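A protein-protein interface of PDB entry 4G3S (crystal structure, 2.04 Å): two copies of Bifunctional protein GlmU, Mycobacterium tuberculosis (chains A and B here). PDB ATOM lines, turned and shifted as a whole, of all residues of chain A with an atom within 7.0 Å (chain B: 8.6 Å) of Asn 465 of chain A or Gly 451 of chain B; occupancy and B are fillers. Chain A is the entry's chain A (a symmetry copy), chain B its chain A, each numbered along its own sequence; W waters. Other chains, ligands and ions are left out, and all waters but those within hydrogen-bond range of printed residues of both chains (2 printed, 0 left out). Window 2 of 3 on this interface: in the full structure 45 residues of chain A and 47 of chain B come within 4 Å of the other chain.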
ATOM      1  N   ILE A 463      -7.445 -21.154  13.229  1.00  0.00           N
ATOM      2  CA  ILE A 463      -6.059 -20.764  13.556  1.00  0.00           C
ATOM      3  C   ILE A 463      -5.317 -20.861  12.240  1.00  0.00           C
ATOM      4  O   ILE A 463      -5.011 -21.952  11.798  1.00  0.00           O
ATOM      5  CB  ILE A 463      -5.439 -21.665  14.645  1.00  0.00           C
ATOM      6  CG1 ILE A 463      -6.336 -21.662  15.914  1.00  0.00           C
ATOM      7  CG2 ILE A 463      -3.987 -21.230  14.974  1.00  0.00           C
ATOM      8  CD1 ILE A 463      -6.126 -22.875  16.828  1.00  0.00           C
ATOM      9  N   GLU A 464      -5.078 -19.746  11.565  1.00  0.00           N
ATOM     10  CA  GLU A 464      -4.384 -19.810  10.256  1.00  0.00           C
ATOM     11  C   GLU A 464      -2.924 -20.334  10.267  1.00  0.00           C
ATOM     12  O   GLU A 464      -2.144 -20.052  11.216  1.00  0.00           O
ATOM     13  CB  GLU A 464      -4.528 -18.487   9.515  1.00  0.00           C
ATOM     14  CG  GLU A 464      -6.002 -18.059   9.422  1.00  0.00           C
ATOM     15  CD  GLU A 464      -6.378 -17.285   8.131  1.00  0.00           C
ATOM     16  OE1 GLU A 464      -5.501 -17.011   7.285  1.00  0.00           O
ATOM     17  OE2 GLU A 464      -7.575 -16.952   7.956  1.00  0.00           O
ATOM     18  N   ASN A 465      -2.563 -21.096   9.213  1.00  0.00           N
ATOM     19  CA  ASN A 465      -1.243 -21.695   9.054  1.00  0.00           C
ATOM     20  C   ASN A 465      -0.768 -22.553  10.219  1.00  0.00           C
ATOM     21  O   ASN A 465       0.444 -22.770  10.366  1.00  0.00           O
ATOM     22  CB  ASN A 465      -0.172 -20.607   8.796  1.00  0.00           C
ATOM     23  CG  ASN A 465      -0.540 -19.681   7.642  1.00  0.00           C
ATOM     24  OD1 ASN A 465      -0.452 -20.071   6.490  1.00  0.00           O
ATOM     25  ND2 ASN A 465      -1.016 -18.477   7.964  1.00  0.00           N
ATOM     26  N   TRP A 466      -1.682 -23.038  11.057  1.00  0.00           N
ATOM     27  CA  TRP A 466      -1.299 -23.903  12.209  1.00  0.00           C
ATOM     28  C   TRP A 466      -0.448 -25.092  11.754  1.00  0.00           C
ATOM     29  O   TRP A 466       0.536 -25.531  12.444  1.00  0.00           O
ATOM     30  CB  TRP A 466      -2.558 -24.436  12.913  1.00  0.00           C
ATOM     31  CG  TRP A 466      -2.267 -25.243  14.128  1.00  0.00           C
ATOM     32  CD1 TRP A 466      -2.037 -24.768  15.393  1.00  0.00           C
ATOM     33  CD2 TRP A 466      -2.162 -26.659  14.200  1.00  0.00           C
ATOM     34  NE1 TRP A 466      -1.787 -25.805  16.266  1.00  0.00           N
ATOM     35  CE2 TRP A 466      -1.847 -26.985  15.558  1.00  0.00           C
ATOM     36  CE3 TRP A 466      -2.255 -27.702  13.234  1.00  0.00           C
ATOM     37  CZ2 TRP A 466      -1.674 -28.312  15.992  1.00  0.00           C
ATOM     38  CZ3 TRP A 466      -2.115 -29.019  13.655  1.00  0.00           C
ATOM     39  CH2 TRP A 466      -1.808 -29.324  15.026  1.00  0.00           C
ATOM     40  N   VAL A 467      -0.885 -25.651  10.612  1.00  0.00           N
ATOM     41  CA  VAL A 467      -0.354 -26.893  10.110  1.00  0.00           C
ATOM     42  C   VAL A 467       1.123 -26.722   9.667  1.00  0.00           C
ATOM     43  O   VAL A 467       1.963 -27.548  10.031  1.00  0.00           O
ATOM     44  CB  VAL A 467      -1.276 -27.534   8.952  1.00  0.00           C
ATOM     45  CG1 VAL A 467      -0.607 -28.742   8.343  1.00  0.00           C
ATOM     46  CG2 VAL A 467      -2.602 -28.013   9.515  1.00  0.00           C
ATOM     47  N   GLN A 468       1.432 -25.647   8.923  1.00  0.00           N
ATOM     48  CA  GLN A 468       2.818 -25.384   8.525  1.00  0.00           C
ATOM     49  C   GLN A 468       3.668 -25.242   9.793  1.00  0.00           C
ATOM     50  O   GLN A 468       4.836 -25.668   9.794  1.00  0.00           O
ATOM     51  CB  GLN A 468       3.026 -24.109   7.666  1.00  0.00           C
ATOM     52  CG  GLN A 468       1.781 -23.484   7.018  1.00  0.00           C
ATOM     53  CD  GLN A 468       1.589 -23.820   5.511  1.00  0.00           C
ATOM     54  OE1 GLN A 468       2.475 -24.401   4.863  1.00  0.00           O
ATOM     55  NE2 GLN A 468       0.414 -23.457   4.965  1.00  0.00           N
ATOM     56  N   ARG A 469       3.092 -24.703  10.877  1.00  0.00           N
ATOM     57  CA  ARG A 469       3.885 -24.458  12.117  1.00  0.00           C
ATOM     58  C   ARG A 469       4.123 -25.703  12.953  1.00  0.00           C
ATOM     59  O   ARG A 469       5.230 -25.922  13.461  1.00  0.00           O
ATOM     60  CB  ARG A 469       3.226 -23.398  13.020  1.00  0.00           C
ATOM     61  CG  ARG A 469       3.417 -21.967  12.569  1.00  0.00           C
ATOM     62  CD  ARG A 469       2.659 -21.092  13.535  1.00  0.00           C
ATOM     63  NE  ARG A 469       1.863 -20.098  12.825  1.00  0.00           N
ATOM     64  CZ  ARG A 469       0.571 -19.845  13.002  1.00  0.00           C
ATOM     65  NH1 ARG A 469      -0.179 -20.491  13.896  1.00  0.00           N
ATOM     66  NH2 ARG A 469       0.037 -18.880  12.265  1.00  0.00           N
ATOM     67  N   LYS A 470       3.062 -26.490  13.109  1.00  0.00           N
ATOM     68  CA  LYS A 470       3.039 -27.592  14.058  1.00  0.00           C
ATOM     69  C   LYS A 470       3.225 -28.974  13.446  1.00  0.00           C
ATOM     70  O   LYS A 470       3.519 -29.923  14.182  1.00  0.00           O
ATOM     71  CB  LYS A 470       1.746 -27.549  14.849  1.00  0.00           C
ATOM     72  CG  LYS A 470       1.591 -26.248  15.684  1.00  0.00           C
ATOM     73  CD  LYS A 470       2.786 -25.967  16.646  1.00  0.00           C
ATOM     74  CE  LYS A 470       3.097 -27.128  17.591  1.00  0.00           C
ATOM     75  NZ  LYS A 470       1.902 -27.606  18.354  1.00  0.00           N
ATOM     76  N   ALA A 476       0.077 -32.959   4.920  1.00  0.00           N
ATOM     77  CA  ALA A 476      -0.874 -31.815   5.113  1.00  0.00           C
ATOM     78  C   ALA A 476      -0.214 -30.413   4.890  1.00  0.00           C
ATOM     79  O   ALA A 476      -0.797 -29.543   4.173  1.00  0.00           O
ATOM     80  CB  ALA A 476      -1.571 -31.909   6.540  1.00  0.00           C
ATOM     81  N   ALA A 477       0.969 -30.189   5.511  1.00  0.00           N
ATOM     82  CA  ALA A 477       1.789 -28.948   5.280  1.00  0.00           C
ATOM     83  C   ALA A 477       2.102 -28.707   3.795  1.00  0.00           C
ATOM     84  O   ALA A 477       1.838 -27.620   3.294  1.00  0.00           O
ATOM     85  CB  ALA A 477       3.127 -28.919   6.156  1.00  0.00           C
ATOM     86  N   ALA A 479       0.515 -29.948   1.124  1.00  0.00           N
ATOM     87  CA  ALA A 479      -0.793 -29.740   0.456  1.00  0.00           C
ATOM     88  C   ALA A 479      -1.320 -28.306   0.635  1.00  0.00           C
ATOM     89  O   ALA A 479      -1.781 -27.708  -0.315  1.00  0.00           O
ATOM     90  CB  ALA A 479      -1.844 -30.785   0.935  1.00  0.00           C
ATOM     91  N   SER A 480      -1.259 -27.763   1.858  1.00  0.00           N
ATOM     92  CA  SER A 480      -1.603 -26.349   2.068  1.00  0.00           C
ATOM     93  C   SER A 480      -0.581 -25.427   1.381  1.00  0.00           C
ATOM     94  O   SER A 480      -1.014 -24.445   0.798  1.00  0.00           O
ATOM     95  CB  SER A 480      -1.705 -25.979   3.558  1.00  0.00           C
ATOM     96  OG  SER A 480      -0.445 -26.133   4.206  1.00  0.00           O
ATOM     97  N   SER B 416      -7.943 -32.451   0.091  1.00  0.00           N
ATOM     98  CA  SER B 416      -6.972 -33.509   0.256  1.00  0.00           C
ATOM     99  C   SER B 416      -6.017 -33.271   1.407  1.00  0.00           C
ATOM    100  O   SER B 416      -5.709 -32.104   1.742  1.00  0.00           O
ATOM    101  CB  SER B 416      -6.151 -33.670  -1.061  1.00  0.00           C
ATOM    102  OG  SER B 416      -7.087 -33.963  -2.122  1.00  0.00           O
ATOM    103  N   HIS B 417      -5.508 -34.367   1.959  1.00  0.00           N
ATOM    104  CA  HIS B 417      -4.507 -34.370   3.026  1.00  0.00           C
ATOM    105  C   HIS B 417      -5.073 -33.685   4.257  1.00  0.00           C
ATOM    106  O   HIS B 417      -4.312 -33.218   5.105  1.00  0.00           O
ATOM    107  CB  HIS B 417      -3.134 -33.732   2.559  1.00  0.00           C
ATOM    108  CG  HIS B 417      -2.564 -34.392   1.354  1.00  0.00           C
ATOM    109  ND1 HIS B 417      -1.856 -35.574   1.422  1.00  0.00           N
ATOM    110  CD2 HIS B 417      -2.686 -34.093   0.033  1.00  0.00           C
ATOM    111  CE1 HIS B 417      -1.508 -35.947   0.200  1.00  0.00           C
ATOM    112  NE2 HIS B 417      -2.006 -35.062  -0.660  1.00  0.00           N
ATOM    113  N   VAL B 418      -6.389 -33.550   4.335  1.00  0.00           N
ATOM    114  CA  VAL B 418      -6.962 -33.098   5.594  1.00  0.00           C
ATOM    115  C   VAL B 418      -6.992 -34.125   6.756  1.00  0.00           C
ATOM    116  O   VAL B 418      -7.090 -35.342   6.511  1.00  0.00           O
ATOM    117  CB  VAL B 418      -8.234 -32.205   5.425  1.00  0.00           C
ATOM    118  CG1 VAL B 418      -8.398 -31.605   4.031  1.00  0.00           C
ATOM    119  CG2 VAL B 418      -9.428 -32.666   6.120  1.00  0.00           C
ATOM    120  N   ILE B 432     -13.628 -27.259   3.560  1.00  0.00           N
ATOM    121  CA  ILE B 432     -12.397 -27.379   4.341  1.00  0.00           C
ATOM    122  C   ILE B 432     -11.310 -27.532   3.322  1.00  0.00           C
ATOM    123  O   ILE B 432     -11.313 -28.509   2.548  1.00  0.00           O
ATOM    124  CB  ILE B 432     -12.367 -28.685   5.219  1.00  0.00           C
ATOM    125  CG1 ILE B 432     -13.698 -28.933   5.947  1.00  0.00           C
ATOM    126  CG2 ILE B 432     -11.083 -28.802   6.075  1.00  0.00           C
ATOM    127  CD1 ILE B 432     -13.955 -28.203   7.148  1.00  0.00           C
ATOM    128  N   GLY B 433     -10.393 -26.547   3.285  1.00  0.00           N
ATOM    129  CA  GLY B 433      -9.216 -26.615   2.430  1.00  0.00           C
ATOM    130  C   GLY B 433      -8.232 -27.734   2.621  1.00  0.00           C
ATOM    131  O   GLY B 433      -8.129 -28.363   3.700  1.00  0.00           O
ATOM    132  N   ASP B 434      -7.455 -27.951   1.565  1.00  0.00           N
ATOM    133  CA  ASP B 434      -6.421 -28.910   1.562  1.00  0.00           C
ATOM    134  C   ASP B 434      -5.501 -28.738   2.747  1.00  0.00           C
ATOM    135  O   ASP B 434      -5.097 -27.604   3.060  1.00  0.00           O
ATOM    136  CB  ASP B 434      -5.566 -28.807   0.291  1.00  0.00           C
ATOM    137  CG  ASP B 434      -6.328 -29.207  -0.988  1.00  0.00           C
ATOM    138  OD1 ASP B 434      -7.476 -29.772  -0.945  1.00  0.00           O
ATOM    139  OD2 ASP B 434      -5.731 -28.990  -2.072  1.00  0.00           O
ATOM    140  N   GLY B 435      -5.151 -29.867   3.372  1.00  0.00           N
ATOM    141  CA  GLY B 435      -4.175 -29.896   4.480  1.00  0.00           C
ATOM    142  C   GLY B 435      -4.674 -29.288   5.788  1.00  0.00           C
ATOM    143  O   GLY B 435      -3.900 -29.268   6.743  1.00  0.00           O
ATOM    144  N   ALA B 436      -5.918 -28.755   5.841  1.00  0.00           N
ATOM    145  CA  ALA B 436      -6.556 -28.303   7.123  1.00  0.00           C
ATOM    146  C   ALA B 436      -6.737 -29.445   8.185  1.00  0.00           C
ATOM    147  O   ALA B 436      -6.699 -30.658   7.857  1.00  0.00           O
ATOM    148  CB  ALA B 436      -7.884 -27.570   6.914  1.00  0.00           C
ATOM    149  N   TYR B 437      -6.858 -29.043   9.458  1.00  0.00           N
ATOM    150  CA  TYR B 437      -7.111 -29.959  10.621  1.00  0.00           C
ATOM    151  C   TYR B 437      -8.324 -29.419  11.350  1.00  0.00           C
ATOM    152  O   TYR B 437      -8.630 -28.204  11.212  1.00  0.00           O
ATOM    153  CB  TYR B 437      -5.963 -29.875  11.609  1.00  0.00           C
ATOM    154  CG  TYR B 437      -4.842 -30.864  11.457  1.00  0.00           C
ATOM    155  CD1 TYR B 437      -4.404 -31.599  12.544  1.00  0.00           C
ATOM    156  CD2 TYR B 437      -4.207 -31.065  10.211  1.00  0.00           C
ATOM    157  CE1 TYR B 437      -3.318 -32.518  12.420  1.00  0.00           C
ATOM    158  CE2 TYR B 437      -3.138 -31.944  10.073  1.00  0.00           C
ATOM    159  CZ  TYR B 437      -2.703 -32.665  11.184  1.00  0.00           C
ATOM    160  OH  TYR B 437      -1.674 -33.557  11.040  1.00  0.00           O
ATOM    161  N   VAL B 448     -12.968 -23.430   6.373  1.00  0.00           N
ATOM    162  CA  VAL B 448     -11.686 -23.550   7.015  1.00  0.00           C
ATOM    163  C   VAL B 448     -10.637 -23.443   5.892  1.00  0.00           C
ATOM    164  O   VAL B 448     -10.588 -24.316   4.973  1.00  0.00           O
ATOM    165  CB  VAL B 448     -11.530 -24.899   7.703  1.00  0.00           C
ATOM    166  CG1 VAL B 448     -10.082 -25.060   8.334  1.00  0.00           C
ATOM    167  CG2 VAL B 448     -12.657 -25.118   8.775  1.00  0.00           C
ATOM    168  N   PRO B 449      -9.741 -22.424   5.972  1.00  0.00           N
ATOM    169  CA  PRO B 449      -8.667 -22.336   4.966  1.00  0.00           C
ATOM    170  C   PRO B 449      -7.750 -23.529   4.902  1.00  0.00           C
ATOM    171  O   PRO B 449      -7.535 -24.200   5.921  1.00  0.00           O
ATOM    172  CB  PRO B 449      -7.825 -21.082   5.432  1.00  0.00           C
ATOM    173  CG  PRO B 449      -8.888 -20.181   5.833  1.00  0.00           C
ATOM    174  CD  PRO B 449      -9.783 -21.192   6.768  1.00  0.00           C
ATOM    175  N   PRO B 450      -7.128 -23.747   3.714  1.00  0.00           N
ATOM    176  CA  PRO B 450      -6.065 -24.680   3.562  1.00  0.00           C
ATOM    177  C   PRO B 450      -5.040 -24.481   4.713  1.00  0.00           C
ATOM    178  O   PRO B 450      -4.724 -23.327   5.101  1.00  0.00           O
ATOM    179  CB  PRO B 450      -5.483 -24.275   2.164  1.00  0.00           C
ATOM    180  CG  PRO B 450      -6.660 -23.909   1.426  1.00  0.00           C
ATOM    181  CD  PRO B 450      -7.365 -23.013   2.440  1.00  0.00           C
ATOM    182  N   GLY B 451      -4.587 -25.577   5.293  1.00  0.00           N
ATOM    183  CA  GLY B 451      -3.550 -25.572   6.361  1.00  0.00           C
ATOM    184  C   GLY B 451      -3.915 -24.868   7.655  1.00  0.00           C
ATOM    185  O   GLY B 451      -3.080 -24.746   8.552  1.00  0.00           O
ATOM    186  N   ALA B 452      -5.168 -24.418   7.779  1.00  0.00           N
ATOM    187  CA  ALA B 452      -5.642 -23.896   9.053  1.00  0.00           C
ATOM    188  C   ALA B 452      -6.108 -25.027  10.006  1.00  0.00           C
ATOM    189  O   ALA B 452      -6.506 -26.146   9.549  1.00  0.00           O
ATOM    190  CB  ALA B 452      -6.806 -22.942   8.785  1.00  0.00           C
ATOM    191  N   LEU B 453      -6.100 -24.723  11.293  1.00  0.00           N
ATOM    192  CA  LEU B 453      -6.735 -25.581  12.295  1.00  0.00           C
ATOM    193  C   LEU B 453      -8.031 -24.896  12.827  1.00  0.00           C
ATOM    194  O   LEU B 453      -7.991 -23.774  13.296  1.00  0.00           O
ATOM    195  CB  LEU B 453      -5.733 -25.940  13.438  1.00  0.00           C
ATOM    196  CG  LEU B 453      -6.286 -26.523  14.747  1.00  0.00           C
ATOM    197  CD1 LEU B 453      -6.846 -27.997  14.624  1.00  0.00           C
ATOM    198  CD2 LEU B 453      -5.297 -26.465  15.967  1.00  0.00           C
ATOM    199  N   ALA B 454      -9.172 -25.568  12.705  1.00  0.00           N
ATOM    200  CA  ALA B 454     -10.444 -25.088  13.231  1.00  0.00           C
ATOM    201  C   ALA B 454     -10.764 -25.795  14.554  1.00  0.00           C
ATOM    202  O   ALA B 454     -10.606 -27.031  14.706  1.00  0.00           O
ATOM    203  CB  ALA B 454     -11.568 -25.282  12.185  1.00  0.00           C
HETATM  204  O   HOH W   1      -4.303 -21.417   7.114  1.00  0.00           O
HETATM  205  O   HOH W   2      -3.253 -28.697  -2.319  1.00  0.00           O
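N of Trp 466 of chain A sits at hydrogen-bond distance from O of Gly 451 of chain B, at 3.3 Å. O of Gly 451 of chain B lies within hydrogen-bond range of N of Val 467 of chain A, at 3.1 Å. The backbone NH (N) of Ile 463 of chain A sits at hydrogen-bond distance from the backbone carbonyl oxygen (O) of Leu 453 of chain B (2.7 Å).
No position is printed for both chains. Of the 17 pairs that touch across the chains among the printed residues, none has its exchanged pair printed and touching as well.
Of the 16 printed residues of chain B, 8 touch a printed residue of chain A. Hydrophobic or aromatic side chains of chain B within 4 Å of the printed part of chain A: His 417, Tyr 437, Ala 452 and Leu 453. Hydrophobic or aromatic side chains of chain A within 4 Å of the printed part of chain B: Ile 463, Trp 466, Val 467, Ala 476 and Ala 479. Among the printed residues, 17 pairs touch across the chains.
Water W2 lies within hydrogen-bond range of OD2 of Asp 434 of chain B and O of Ala 479 of chain A. Water W1 lies within hydrogen-bond range of the backbone NH of Asn 465 of chain A (2.7 Å), the backbone carbonyl oxygen of Pro 450 of chain B (2.8 Å) and the backbone NH of Ala 452 of chain B (3.2 Å).
The backbone NH (N) of Ser 416 of chain B sits at hydrogen-bond distance from the side-chain carboxylate (OD1) of Asp 434 of chain B. The backbone NH (N) of Gly 435 of chain B lies within hydrogen-bond range of the backbone carbonyl oxygen (O) of Ser 416 of chain B (2.8 Å). O of Ala 452 of chain B lies within hydrogen-bond range of N of Tyr 437 of chain B, 2.9 Å away. NE2 of Gln 468 of chain A lies within hydrogen-bond range of OG of Ser 480 of chain A, 2.9 Å away. O of Ala 476 of chain A sits at hydrogen-bond distance from OG of Ser 480 of chain A (3.4 Å). The backbone carbonyl oxygen (O) of Ala 477 of chain A is in hydrogen-bond range of the side-chain hydroxyl (OG) of Ser 480 of chain A, 2.9 Å away.
O of Ile 463 of chain A touches CA of Ala 452 of chain B, 3.4 Å away. Asn 465 of chain A touches Gly 451 of chain B. CE2 of Trp 466 of chain A touches CD2 of Leu 453 of chain B, at 3.5 Å. Gly 435 of chain B touches Val 467 of chain A. Ala 476 of chain A touches His 417 of chain B. Gly 435 of chain B touches Ala 476 of chain A. CB of Ala 476 of chain A touches CE2 of Tyr 437 of chain B, 3.9 Å away. CB of Asp 434 of chain B touches O of Ala 479 of chain A (3.99 Å). O of Asp 434 of chain B touches CB of Ser 480 of chain A (3.8 Å). CB of Ser 480 of chain A touches CA of Gly 451 of chain B (3.4 Å).
Gly 451 of chain B touches just these residues of chain A: Asn 465 (3.6 Å), Trp 466 (3.3 Å), Val 467 (3.1 Å) and Ser 480 (3.4 Å). Printed residues of chain B within 4 Å of Trp 466 of chain A: Tyr 437 (3.6 Å), Gly 451 (3.3 Å) and Leu 453 (3.5 Å). Printed residues of chain A within 4 Å of Tyr 437 of chain B: Trp 466, Val 467 and Ala 476. Of the printed residues of chain B, Val 467 of chain A touches Gly 435, Tyr 437 and Gly 451. Val 418 of chain B touches none of the printed residues of chain A. The nearest residue of chain B that does not touch Asn 465 of chain A is Ala 452 of chain B (4.2 Å). The nearest residue of chain A that does not touch Gly 451 of chain B is Gln 468 of chain A (4.6 Å). The nearest printed residue of chain A that does not touch Leu 453 of chain B is Glu 464 of chain A (5.1 Å).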
